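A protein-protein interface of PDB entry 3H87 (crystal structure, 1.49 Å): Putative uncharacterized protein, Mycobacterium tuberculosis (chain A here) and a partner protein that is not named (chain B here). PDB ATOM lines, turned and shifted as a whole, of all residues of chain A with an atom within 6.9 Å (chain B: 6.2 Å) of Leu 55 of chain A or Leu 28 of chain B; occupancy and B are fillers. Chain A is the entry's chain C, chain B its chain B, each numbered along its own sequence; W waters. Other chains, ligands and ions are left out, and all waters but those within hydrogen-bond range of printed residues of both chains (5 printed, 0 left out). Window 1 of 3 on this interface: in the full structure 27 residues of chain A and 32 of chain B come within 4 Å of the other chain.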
ATOM      1  N   ALA A  50      16.564   5.407  13.982  1.00  0.00           N
ATOM      2  CA  ALA A  50      17.799   5.189  14.735  1.00  0.00           C
ATOM      3  C   ALA A  50      17.903   3.743  15.217  1.00  0.00           C
ATOM      4  O   ALA A  50      19.008   3.183  15.296  1.00  0.00           O
ATOM      5  CB  ALA A  50      17.875   6.162  15.974  1.00  0.00           C
ATOM      6  N   ASP A  51      16.769   3.126  15.564  1.00  0.00           N
ATOM      7  CA  ASP A  51      16.771   1.712  15.976  1.00  0.00           C
ATOM      8  C   ASP A  51      17.239   0.824  14.812  1.00  0.00           C
ATOM      9  O   ASP A  51      18.052  -0.108  15.008  1.00  0.00           O
ATOM     10  CB  ASP A  51      15.366   1.257  16.414  1.00  0.00           C
ATOM     11  CG  ASP A  51      14.873   1.868  17.690  1.00  0.00           C
ATOM     12  OD1 ASP A  51      15.662   2.017  18.656  1.00  0.00           O
ATOM     13  OD2 ASP A  51      13.637   2.170  17.766  1.00  0.00           O
ATOM     14  N   LEU A  52      16.728   1.086  13.604  1.00  0.00           N
ATOM     15  CA  LEU A  52      17.157   0.292  12.441  1.00  0.00           C
ATOM     16  C   LEU A  52      18.646   0.482  12.133  1.00  0.00           C
ATOM     17  O   LEU A  52      19.300  -0.480  11.686  1.00  0.00           O
ATOM     18  CB  LEU A  52      16.301   0.614  11.205  1.00  0.00           C
ATOM     19  CG  LEU A  52      14.826   0.311  11.341  1.00  0.00           C
ATOM     20  CD1 LEU A  52      14.083   0.596  10.035  1.00  0.00           C
ATOM     21  CD2 LEU A  52      14.518  -1.085  11.804  1.00  0.00           C
ATOM     22  N   ARG A  53      19.179   1.693  12.296  1.00  0.00           N
ATOM     23  CA  ARG A  53      20.608   1.960  12.041  1.00  0.00           C
ATOM     24  C   ARG A  53      21.453   1.262  13.117  1.00  0.00           C
ATOM     25  O   ARG A  53      22.525   0.686  12.797  1.00  0.00           O
ATOM     26  CB  ARG A  53      20.820   3.478  12.053  1.00  0.00           C
ATOM     27  CG  ARG A  53      22.122   3.985  11.522  1.00  0.00           C
ATOM     28  CD  ARG A  53      21.961   5.448  10.989  1.00  0.00           C
ATOM     29  NE  ARG A  53      21.032   6.270  11.770  1.00  0.00           N
ATOM     30  CZ  ARG A  53      19.880   6.786  11.319  1.00  0.00           C
ATOM     31  NH1 ARG A  53      19.477   6.596  10.057  1.00  0.00           N
ATOM     32  NH2 ARG A  53      19.133   7.520  12.128  1.00  0.00           N
ATOM     33  N   ARG A  54      21.013   1.278  14.388  1.00  0.00           N
ATOM     34  CA  ARG A  54      21.741   0.577  15.476  1.00  0.00           C
ATOM     35  C   ARG A  54      21.817  -0.907  15.166  1.00  0.00           C
ATOM     36  O   ARG A  54      22.883  -1.542  15.266  1.00  0.00           O
ATOM     37  CB  ARG A  54      21.051   0.791  16.835  1.00  0.00           C
ATOM     38  CG  ARG A  54      21.850   0.263  18.020  1.00  0.00           C
ATOM     39  CD  ARG A  54      21.004   0.015  19.293  1.00  0.00           C
ATOM     40  NE  ARG A  54      20.126  -1.095  19.013  1.00  0.00           N
ATOM     41  CZ  ARG A  54      18.799  -1.033  18.859  1.00  0.00           C
ATOM     42  NH1 ARG A  54      18.116   0.067  19.133  1.00  0.00           N
ATOM     43  NH2 ARG A  54      18.206  -2.085  18.411  1.00  0.00           N
ATOM     44  N   LEU A  55      20.685  -1.484  14.745  1.00  0.00           N
ATOM     45  CA  LEU A  55      20.667  -2.897  14.411  1.00  0.00           C
ATOM     46  C   LEU A  55      21.651  -3.207  13.282  1.00  0.00           C
ATOM     47  O   LEU A  55      22.434  -4.159  13.387  1.00  0.00           O
ATOM     48  CB  LEU A  55      19.256  -3.347  13.981  1.00  0.00           C
ATOM     49  CG  LEU A  55      19.165  -4.841  13.592  1.00  0.00           C
ATOM     50  CD1 LEU A  55      19.538  -5.858  14.649  1.00  0.00           C
ATOM     51  CD2 LEU A  55      17.790  -5.156  13.054  1.00  0.00           C
ATOM     52  N   ARG A  56      21.669  -2.386  12.224  1.00  0.00           N
ATOM     53  CA  ARG A  56      22.567  -2.659  11.098  1.00  0.00           C
ATOM     54  C   ARG A  56      24.021  -2.687  11.542  1.00  0.00           C
ATOM     55  O   ARG A  56      24.795  -3.516  11.076  1.00  0.00           O
ATOM     56  CB  ARG A  56      22.356  -1.627   9.995  1.00  0.00           C
ATOM     57  CG  ARG A  56      23.096  -1.963   8.728  1.00  0.00           C
ATOM     58  CD  ARG A  56      24.494  -1.383   8.712  1.00  0.00           C
ATOM     59  NE  ARG A  56      24.482   0.048   8.486  1.00  0.00           N
ATOM     60  CZ  ARG A  56      24.337   0.623   7.292  1.00  0.00           C
ATOM     61  NH1 ARG A  56      24.163  -0.120   6.204  1.00  0.00           N
ATOM     62  NH2 ARG A  56      24.345   1.945   7.187  1.00  0.00           N
ATOM     63  N   GLY A  57      24.394  -1.784  12.446  1.00  0.00           N
ATOM     64  CA  GLY A  57      25.777  -1.804  12.916  1.00  0.00           C
ATOM     65  C   GLY A  57      26.112  -3.050  13.708  1.00  0.00           C
ATOM     66  O   GLY A  57      27.237  -3.544  13.645  1.00  0.00           O
ATOM     67  N   ALA A  58      25.153  -3.581  14.443  1.00  0.00           N
ATOM     68  CA  ALA A  58      25.380  -4.768  15.242  1.00  0.00           C
ATOM     69  C   ALA A  58      25.403  -6.064  14.441  1.00  0.00           C
ATOM     70  O   ALA A  58      26.096  -7.006  14.822  1.00  0.00           O
ATOM     71  CB  ALA A  58      24.258  -4.861  16.289  1.00  0.00           C
ATOM     72  N   VAL A  59      24.620  -6.120  13.363  1.00  0.00           N
ATOM     73  CA  VAL A  59      24.456  -7.361  12.558  1.00  0.00           C
ATOM     74  C   VAL A  59      25.018  -7.234  11.135  1.00  0.00           C
ATOM     75  O   VAL A  59      24.614  -7.985  10.219  1.00  0.00           O
ATOM     76  CB  VAL A  59      22.935  -7.830  12.487  1.00  0.00           C
ATOM     77  CG1 VAL A  59      22.355  -7.989  13.894  1.00  0.00           C
ATOM     78  CG2 VAL A  59      22.072  -6.909  11.668  1.00  0.00           C
ATOM     79  N   ALA A  60      25.973  -6.335  10.913  1.00  0.00           N
ATOM     80  CA  ALA A  60      26.505  -6.122   9.590  1.00  0.00           C
ATOM     81  C   ALA A  60      26.971  -7.428   8.951  1.00  0.00           C
ATOM     82  O   ALA A  60      26.882  -7.608   7.713  1.00  0.00           O
ATOM     83  CB  ALA A  60      27.673  -5.143   9.675  1.00  0.00           C
ATOM     84  N   LEU A  62      25.599 -10.211   8.710  1.00  0.00           N
ATOM     85  CA  LEU A  62      24.542 -10.889   7.926  1.00  0.00           C
ATOM     86  C   LEU A  62      24.689 -10.631   6.435  1.00  0.00           C
ATOM     87  O   LEU A  62      24.185 -11.403   5.614  1.00  0.00           O
ATOM     88  CB  LEU A  62      23.163 -10.428   8.384  1.00  0.00           C
ATOM     89  CG  LEU A  62      22.688 -10.800   9.765  1.00  0.00           C
ATOM     90  CD1 LEU A  62      21.335 -10.157  10.051  1.00  0.00           C
ATOM     91  CD2 LEU A  62      22.649 -12.337   9.953  1.00  0.00           C
ATOM     92  N   ILE B  23      10.516 -11.726   7.624  1.00  0.00           N
ATOM     93  CA  ILE B  23      11.720 -11.018   7.176  1.00  0.00           C
ATOM     94  C   ILE B  23      12.944 -11.939   7.182  1.00  0.00           C
ATOM     95  O   ILE B  23      13.318 -12.492   8.199  1.00  0.00           O
ATOM     96  CB  ILE B  23      11.978  -9.687   7.940  1.00  0.00           C
ATOM     97  CG1 ILE B  23      13.020  -8.827   7.198  1.00  0.00           C
ATOM     98  CG2 ILE B  23      12.349  -9.945   9.431  1.00  0.00           C
ATOM     99  CD1 ILE B  23      13.133  -7.388   7.750  1.00  0.00           C
ATOM    100  N   ASP B  24      13.594 -12.046   6.021  1.00  0.00           N
ATOM    101  CA  ASP B  24      14.839 -12.800   5.903  1.00  0.00           C
ATOM    102  C   ASP B  24      16.046 -11.956   6.341  1.00  0.00           C
ATOM    103  O   ASP B  24      15.982 -10.712   6.293  1.00  0.00           O
ATOM    104  CB  ASP B  24      15.065 -13.171   4.431  1.00  0.00           C
ATOM    105  CG  ASP B  24      16.264 -14.065   4.243  1.00  0.00           C
ATOM    106  OD1 ASP B  24      16.212 -15.194   4.793  1.00  0.00           O
ATOM    107  OD2 ASP B  24      17.242 -13.697   3.542  1.00  0.00           O
ATOM    108  N   LYS B  25      17.157 -12.600   6.720  1.00  0.00           N
ATOM    109  CA  LYS B  25      18.370 -11.859   7.072  1.00  0.00           C
ATOM    110  C   LYS B  25      18.790 -10.851   6.023  1.00  0.00           C
ATOM    111  O   LYS B  25      19.339  -9.772   6.360  1.00  0.00           O
ATOM    112  CB  LYS B  25      19.558 -12.795   7.375  1.00  0.00           C
ATOM    113  CG  LYS B  25      19.996 -13.734   6.195  1.00  0.00           C
ATOM    114  CD  LYS B  25      21.283 -14.457   6.522  1.00  0.00           C
ATOM    115  CE  LYS B  25      21.702 -15.466   5.448  1.00  0.00           C
ATOM    116  NZ  LYS B  25      20.756 -16.658   5.423  1.00  0.00           N
ATOM    117  N   SER B  26      18.576 -11.168   4.737  1.00  0.00           N
ATOM    118  CA  SER B  26      19.038 -10.330   3.633  1.00  0.00           C
ATOM    119  C   SER B  26      18.335  -8.996   3.594  1.00  0.00           C
ATOM    120  O   SER B  26      18.933  -7.973   3.190  1.00  0.00           O
ATOM    121  CB  SER B  26      18.923 -11.068   2.295  1.00  0.00           C
ATOM    122  OG  SER B  26      17.572 -11.462   2.054  1.00  0.00           O
ATOM    123  N   ALA B  27      17.078  -8.954   4.019  1.00  0.00           N
ATOM    124  CA  ALA B  27      16.345  -7.673   4.132  1.00  0.00           C
ATOM    125  C   ALA B  27      16.620  -7.013   5.482  1.00  0.00           C
ATOM    126  O   ALA B  27      16.730  -5.768   5.561  1.00  0.00           O
ATOM    127  CB  ALA B  27      14.826  -7.870   3.949  1.00  0.00           C
ATOM    128  N   LEU B  28      16.723  -7.800   6.567  1.00  0.00           N
ATOM    129  CA  LEU B  28      16.930  -7.221   7.901  1.00  0.00           C
ATOM    130  C   LEU B  28      18.153  -6.296   7.937  1.00  0.00           C
ATOM    131  O   LEU B  28      18.091  -5.187   8.489  1.00  0.00           O
ATOM    132  CB  LEU B  28      17.063  -8.406   8.888  1.00  0.00           C
ATOM    133  CG  LEU B  28      17.145  -8.016  10.346  1.00  0.00           C
ATOM    134  CD1 LEU B  28      15.800  -7.433  10.865  1.00  0.00           C
ATOM    135  CD2 LEU B  28      17.561  -9.232  11.189  1.00  0.00           C
ATOM    136  N   VAL B  29      19.257  -6.721   7.342  1.00  0.00           N
ATOM    137  CA  VAL B  29      20.504  -5.968   7.392  1.00  0.00           C
ATOM    138  C   VAL B  29      20.487  -4.772   6.421  1.00  0.00           C
ATOM    139  O   VAL B  29      21.321  -3.858   6.555  1.00  0.00           O
ATOM    140  CB  VAL B  29      21.739  -6.915   7.155  1.00  0.00           C
ATOM    141  CG1 VAL B  29      21.841  -7.387   5.719  1.00  0.00           C
ATOM    142  CG2 VAL B  29      23.049  -6.290   7.628  1.00  0.00           C
ATOM    143  N   ARG B  30      19.530  -4.707   5.490  1.00  0.00           N
ATOM    144  CA  ARG B  30      19.467  -3.649   4.467  1.00  0.00           C
ATOM    145  C   ARG B  30      18.322  -2.651   4.675  1.00  0.00           C
ATOM    146  O   ARG B  30      18.239  -1.690   3.912  1.00  0.00           O
ATOM    147  CB  ARG B  30      19.372  -4.315   3.077  1.00  0.00           C
ATOM    148  CG  ARG B  30      20.668  -5.031   2.698  1.00  0.00           C
ATOM    149  CD  ARG B  30      20.616  -5.734   1.330  1.00  0.00           C
ATOM    150  NE  ARG B  30      21.881  -6.357   0.954  1.00  0.00           N
ATOM    151  CZ  ARG B  30      22.308  -7.554   1.360  1.00  0.00           C
ATOM    152  NH1 ARG B  30      21.601  -8.310   2.157  1.00  0.00           N
ATOM    153  NH2 ARG B  30      23.493  -8.024   0.961  1.00  0.00           N
ATOM    154  N   LEU B  31      17.492  -2.805   5.702  1.00  0.00           N
ATOM    155  CA  LEU B  31      16.352  -1.880   5.931  1.00  0.00           C
ATOM    156  C   LEU B  31      16.811  -0.422   5.988  1.00  0.00           C
ATOM    157  O   LEU B  31      16.170   0.449   5.408  1.00  0.00           O
ATOM    158  CB  LEU B  31      15.618  -2.234   7.242  1.00  0.00           C
ATOM    159  CG  LEU B  31      14.831  -3.520   7.274  1.00  0.00           C
ATOM    160  CD1 LEU B  31      14.285  -3.763   8.715  1.00  0.00           C
ATOM    161  CD2 LEU B  31      13.679  -3.502   6.274  1.00  0.00           C
ATOM    162  N   THR B  32      17.882  -0.155   6.725  1.00  0.00           N
ATOM    163  CA  THR B  32      18.241   1.220   7.009  1.00  0.00           C
ATOM    164  C   THR B  32      18.630   1.890   5.706  1.00  0.00           C
ATOM    165  O   THR B  32      18.521   3.155   5.674  1.00  0.00           O
ATOM    166  CB  THR B  32      19.380   1.264   8.080  1.00  0.00           C
ATOM    167  OG1 THR B  32      19.591   2.605   8.551  1.00  0.00           O
ATOM    168  CG2 THR B  32      20.682   0.692   7.443  1.00  0.00           C
ATOM    169  N   ILE B  51       9.553 -12.882  12.344  1.00  0.00           N
ATOM    170  CA  ILE B  51      10.944 -13.342  12.192  1.00  0.00           C
ATOM    171  C   ILE B  51      11.018 -14.781  12.685  1.00  0.00           C
ATOM    172  O   ILE B  51      10.337 -15.142  13.668  1.00  0.00           O
ATOM    173  CB  ILE B  51      11.940 -12.426  12.912  1.00  0.00           C
ATOM    174  CG1 ILE B  51      13.396 -12.715  12.497  1.00  0.00           C
ATOM    175  CG2 ILE B  51      11.781 -12.513  14.414  1.00  0.00           C
ATOM    176  CD1 ILE B  51      14.408 -11.670  13.029  1.00  0.00           C
ATOM    177  N   THR B  55      16.430 -17.303  11.890  1.00  0.00           N
ATOM    178  CA  THR B  55      17.011 -15.970  11.601  1.00  0.00           C
ATOM    179  C   THR B  55      17.558 -15.314  12.888  1.00  0.00           C
ATOM    180  O   THR B  55      18.584 -14.643  12.854  1.00  0.00           O
ATOM    181  CB  THR B  55      15.989 -15.059  10.888  1.00  0.00           C
ATOM    182  OG1 THR B  55      15.509 -15.749   9.703  1.00  0.00           O
ATOM    183  CG2 THR B  55      16.579 -13.699  10.494  1.00  0.00           C
ATOM    184  N   VAL B  59      21.279 -13.757  13.482  1.00  0.00           N
ATOM    185  CA  VAL B  59      21.576 -12.491  14.197  1.00  0.00           C
ATOM    186  C   VAL B  59      22.619 -12.722  15.293  1.00  0.00           C
ATOM    187  O   VAL B  59      23.615 -11.991  15.384  1.00  0.00           O
ATOM    188  CB  VAL B  59      20.306 -11.894  14.770  1.00  0.00           C
ATOM    189  CG1 VAL B  59      20.607 -10.765  15.789  1.00  0.00           C
ATOM    190  CG2 VAL B  59      19.401 -11.393  13.648  1.00  0.00           C
ATOM    191  N   ARG B  71      21.308  -7.219  23.801  1.00  0.00           N
ATOM    192  CA  ARG B  71      20.729  -5.882  23.551  1.00  0.00           C
ATOM    193  C   ARG B  71      19.800  -5.834  22.364  1.00  0.00           C
ATOM    194  O   ARG B  71      18.667  -5.317  22.429  1.00  0.00           O
ATOM    195  CB  ARG B  71      21.845  -4.858  23.367  1.00  0.00           C
ATOM    196  CG  ARG B  71      21.361  -3.385  23.173  1.00  0.00           C
ATOM    197  CD  ARG B  71      22.490  -2.483  22.687  1.00  0.00           C
ATOM    198  NE  ARG B  71      22.779  -2.728  21.271  1.00  0.00           N
ATOM    199  CZ  ARG B  71      23.914  -2.399  20.656  1.00  0.00           C
ATOM    200  NH1 ARG B  71      24.906  -1.852  21.319  1.00  0.00           N
ATOM    201  NH2 ARG B  71      24.071  -2.631  19.369  1.00  0.00           N
ATOM    202  N   GLU B  72      20.245  -6.361  21.240  1.00  0.00           N
ATOM    203  CA  GLU B  72      19.369  -6.351  20.083  1.00  0.00           C
ATOM    204  C   GLU B  72      18.080  -7.090  20.342  1.00  0.00           C
ATOM    205  O   GLU B  72      16.969  -6.629  19.920  1.00  0.00           O
ATOM    206  CB  GLU B  72      20.076  -6.911  18.858  1.00  0.00           C
ATOM    207  CG  GLU B  72      21.191  -5.984  18.367  1.00  0.00           C
ATOM    208  CD  GLU B  72      20.717  -4.535  18.154  1.00  0.00           C
ATOM    209  OE1 GLU B  72      19.647  -4.363  17.525  1.00  0.00           O
ATOM    210  OE2 GLU B  72      21.402  -3.587  18.617  1.00  0.00           O
ATOM    211  N   PRO B  76      13.708  -2.599  20.153  1.00  0.00           N
ATOM    212  CA  PRO B  76      13.189  -2.508  18.759  1.00  0.00           C
ATOM    213  C   PRO B  76      14.378  -2.394  17.801  1.00  0.00           C
ATOM    214  O   PRO B  76      15.375  -1.755  18.173  1.00  0.00           O
ATOM    215  CB  PRO B  76      12.326  -1.248  18.787  1.00  0.00           C
ATOM    216  CG  PRO B  76      12.813  -0.465  19.952  1.00  0.00           C
ATOM    217  CD  PRO B  76      13.387  -1.403  20.951  1.00  0.00           C
ATOM    218  N   PRO B  77      14.267  -2.907  16.574  1.00  0.00           N
ATOM    219  CA  PRO B  77      13.084  -3.547  16.008  1.00  0.00           C
ATOM    220  C   PRO B  77      12.826  -5.000  16.391  1.00  0.00           C
ATOM    221  O   PRO B  77      11.656  -5.452  16.296  1.00  0.00           O
ATOM    222  CB  PRO B  77      13.360  -3.459  14.504  1.00  0.00           C
ATOM    223  CG  PRO B  77      14.839  -3.628  14.418  1.00  0.00           C
ATOM    224  CD  PRO B  77      15.336  -2.753  15.561  1.00  0.00           C
ATOM    225  N   LEU B  78      13.846  -5.769  16.818  1.00  0.00           N
ATOM    226  CA  LEU B  78      13.638  -7.199  16.950  1.00  0.00           C
ATOM    227  C   LEU B  78      12.585  -7.500  17.996  1.00  0.00           C
ATOM    228  O   LEU B  78      11.830  -8.469  17.834  1.00  0.00           O
ATOM    229  CB  LEU B  78      14.933  -7.946  17.272  1.00  0.00           C
ATOM    230  CG  LEU B  78      15.995  -7.900  16.150  1.00  0.00           C
ATOM    231  CD1 LEU B  78      17.282  -8.642  16.553  1.00  0.00           C
ATOM    232  CD2 LEU B  78      15.528  -8.450  14.803  1.00  0.00           C
ATOM    233  N   MET B  81       8.992  -7.918  16.641  1.00  0.00           N
ATOM    234  CA  MET B  81       8.687  -8.891  15.559  1.00  0.00           C
ATOM    235  C   MET B  81       8.185 -10.227  16.147  1.00  0.00           C
ATOM    236  O   MET B  81       8.958 -10.920  16.838  1.00  0.00           O
ATOM    237  CB  MET B  81       9.958  -9.158  14.775  1.00  0.00           C
ATOM    238  CG  MET B  81      10.436  -7.942  13.966  1.00  0.00           C
ATOM    239  SD  MET B  81      12.014  -8.267  13.103  1.00  0.00           S
ATOM    240  CE  MET B  81      12.194  -6.731  12.144  1.00  0.00           C
ATOM    241  N   LEU B 129      10.009 -11.344   2.876  1.00  0.00           N
ATOM    242  CA  LEU B 129      10.667 -10.075   2.569  1.00  0.00           C
ATOM    243  C   LEU B 129      12.155 -10.301   2.542  1.00  0.00           C
ATOM    244  O   LEU B 129      12.741 -10.777   3.540  1.00  0.00           O
ATOM    245  CB  LEU B 129      10.297  -9.010   3.640  1.00  0.00           C
ATOM    246  CG  LEU B 129      10.909  -7.637   3.469  1.00  0.00           C
ATOM    247  CD1 LEU B 129      10.457  -6.989   2.174  1.00  0.00           C
ATOM    248  CD2 LEU B 129      10.625  -6.720   4.727  1.00  0.00           C
ATOM    249  N   LEU B 149      12.900  -6.114  -0.997  1.00  0.00           N
ATOM    250  CA  LEU B 149      13.103  -4.794  -0.387  1.00  0.00           C
ATOM    251  C   LEU B 149      13.724  -3.831  -1.395  1.00  0.00           C
ATOM    252  O   LEU B 149      14.723  -4.151  -2.068  1.00  0.00           O
ATOM    253  CB  LEU B 149      14.039  -4.945   0.801  1.00  0.00           C
ATOM    254  CG  LEU B 149      14.421  -3.694   1.594  1.00  0.00           C
ATOM    255  CD1 LEU B 149      13.175  -3.113   2.297  1.00  0.00           C
ATOM    256  CD2 LEU B 149      15.534  -3.994   2.557  1.00  0.00           C
HETATM  257  O   HOH W   1      23.449  -3.018   5.093  1.00  0.00           O
HETATM  258  O   HOH W   2      18.650  -2.275   9.107  1.00  0.00           O
HETATM  259  O   HOH W   3      16.701  -4.904  17.680  1.00  0.00           O
HETATM  260  O   HOH W   4      17.433   3.818   9.502  1.00  0.00           O
HETATM  261  O   HOH W   5      22.330 -10.988   3.465  1.00  0.00           O
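OD1 of Asp 51 of chain A is in salt-bridge range of NH1 of Arg 54 of chain A (3.2 Å). The side-chain carboxylate (OE2) of Glu 72 of chain B is in salt-bridge range of the guanidinium group (NH2) of Arg 71 of chain B, 2.9 Å away.
Water W4 bridges the side-chain hydroxyl of Thr 32 of chain B and the guanidinium group of Arg 53 of chain A. Water W1 lies within hydrogen-bond range of the backbone carbonyl oxygen of Val 29 of chain B (2.7 Å) and the guanidinium group of Arg 56 of chain A (3.2 Å). Water W3 lies within hydrogen-bond range of the backbone carbonyl oxygen (O) of Glu 72 of chain B (2.8 Å), the backbone NH (N) of Leu 78 of chain B (3.1 Å), the guanidinium group (NH2) of Arg 54 of chain A (3.3 Å) and the backbone carbonyl oxygen (O) of Pro 76 of chain B (3.5 Å). Water W5 bridges O of Leu 62 of chain A (2.9 Å) and NH1 of Arg 30 of chain B (3.1 Å). Water W2 lies within hydrogen-bond range of O of Leu 28 of chain B, O of Leu 52 of chain A and N of Thr 32 of chain B.
Of the 12 printed residues of chain A, 10 touch a printed residue of chain B. Printed residues of chain A that touch a printed residue of chain B: Asp 51, Leu 52, Arg 53, Arg 54, Leu 55, Arg 56, Ala 58, Val 59, Ala 60 and Leu 62. Hydrophobic or aromatic side chains of chain A within 4 Å of the printed part of chain B: Leu 52, Leu 55, Ala 58, Val 59 and Leu 62. Among the printed residues, 18 pairs touch across the chains.
The backbone carbonyl oxygen (O) of Pro 76 of chain B sits at hydrogen-bond distance from the guanidinium group (NH2) of Arg 54 of chain A, at 2.9 Å. The side-chain carboxylate (OE2) of Glu 72 of chain B is in salt-bridge range of the guanidinium group (NE) of Arg 54 of chain A.
CB of Asp 51 of chain A touches O of Pro 76 of chain B (3.5 Å). Pro 77 of chain B touches Leu 52 of chain A (CG to CD2, 3.7 Å). Arg 53 of chain A touches Thr 32 of chain B (CA to OG1, 3.7 Å). Arg 71 of chain B touches Arg 54 of chain A. Leu 28 of chain B touches Leu 55 of chain A. OE1 of Glu 72 of chain B touches CD1 of Leu 55 of chain A, 3.2 Å away. Arg 56 of chain A touches Val 29 of chain B (CG to O, 3.4 Å). CB of Ala 58 of chain A touches NH2 of Arg 71 of chain B, at 3.8 Å. Val 59 of chain B touches Val 59 of chain A (CG1 to CG1, 3.8 Å). Val 29 of chain B touches Ala 60 of chain A (CG2 to CA, 3.98 Å).
Of chain B, only Leu 28 (3.7 Å), Glu 72 (3.2 Å) and Pro 77 (3.6 Å) come within 4 Å of Leu 55 of chain A. Leu 28 of chain B touches one residue of chain A. Printed residues of chain B within 4 Å of Arg 54 of chain A: Arg 71, Glu 72 and Pro 76. Printed residues of chain B within 4 Å of Leu 62 of chain A: Val 29 (3.98 Å). Of the printed residues of chain A, Arg 71 of chain B touches Arg 54 (3.8 Å) and Ala 58 (3.8 Å). Met 81 of chain B touches none of the printed residues of chain A. The nearest residue of chain A that does not touch Leu 28 of chain B is Leu 62 of chain A (4.05 Å).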
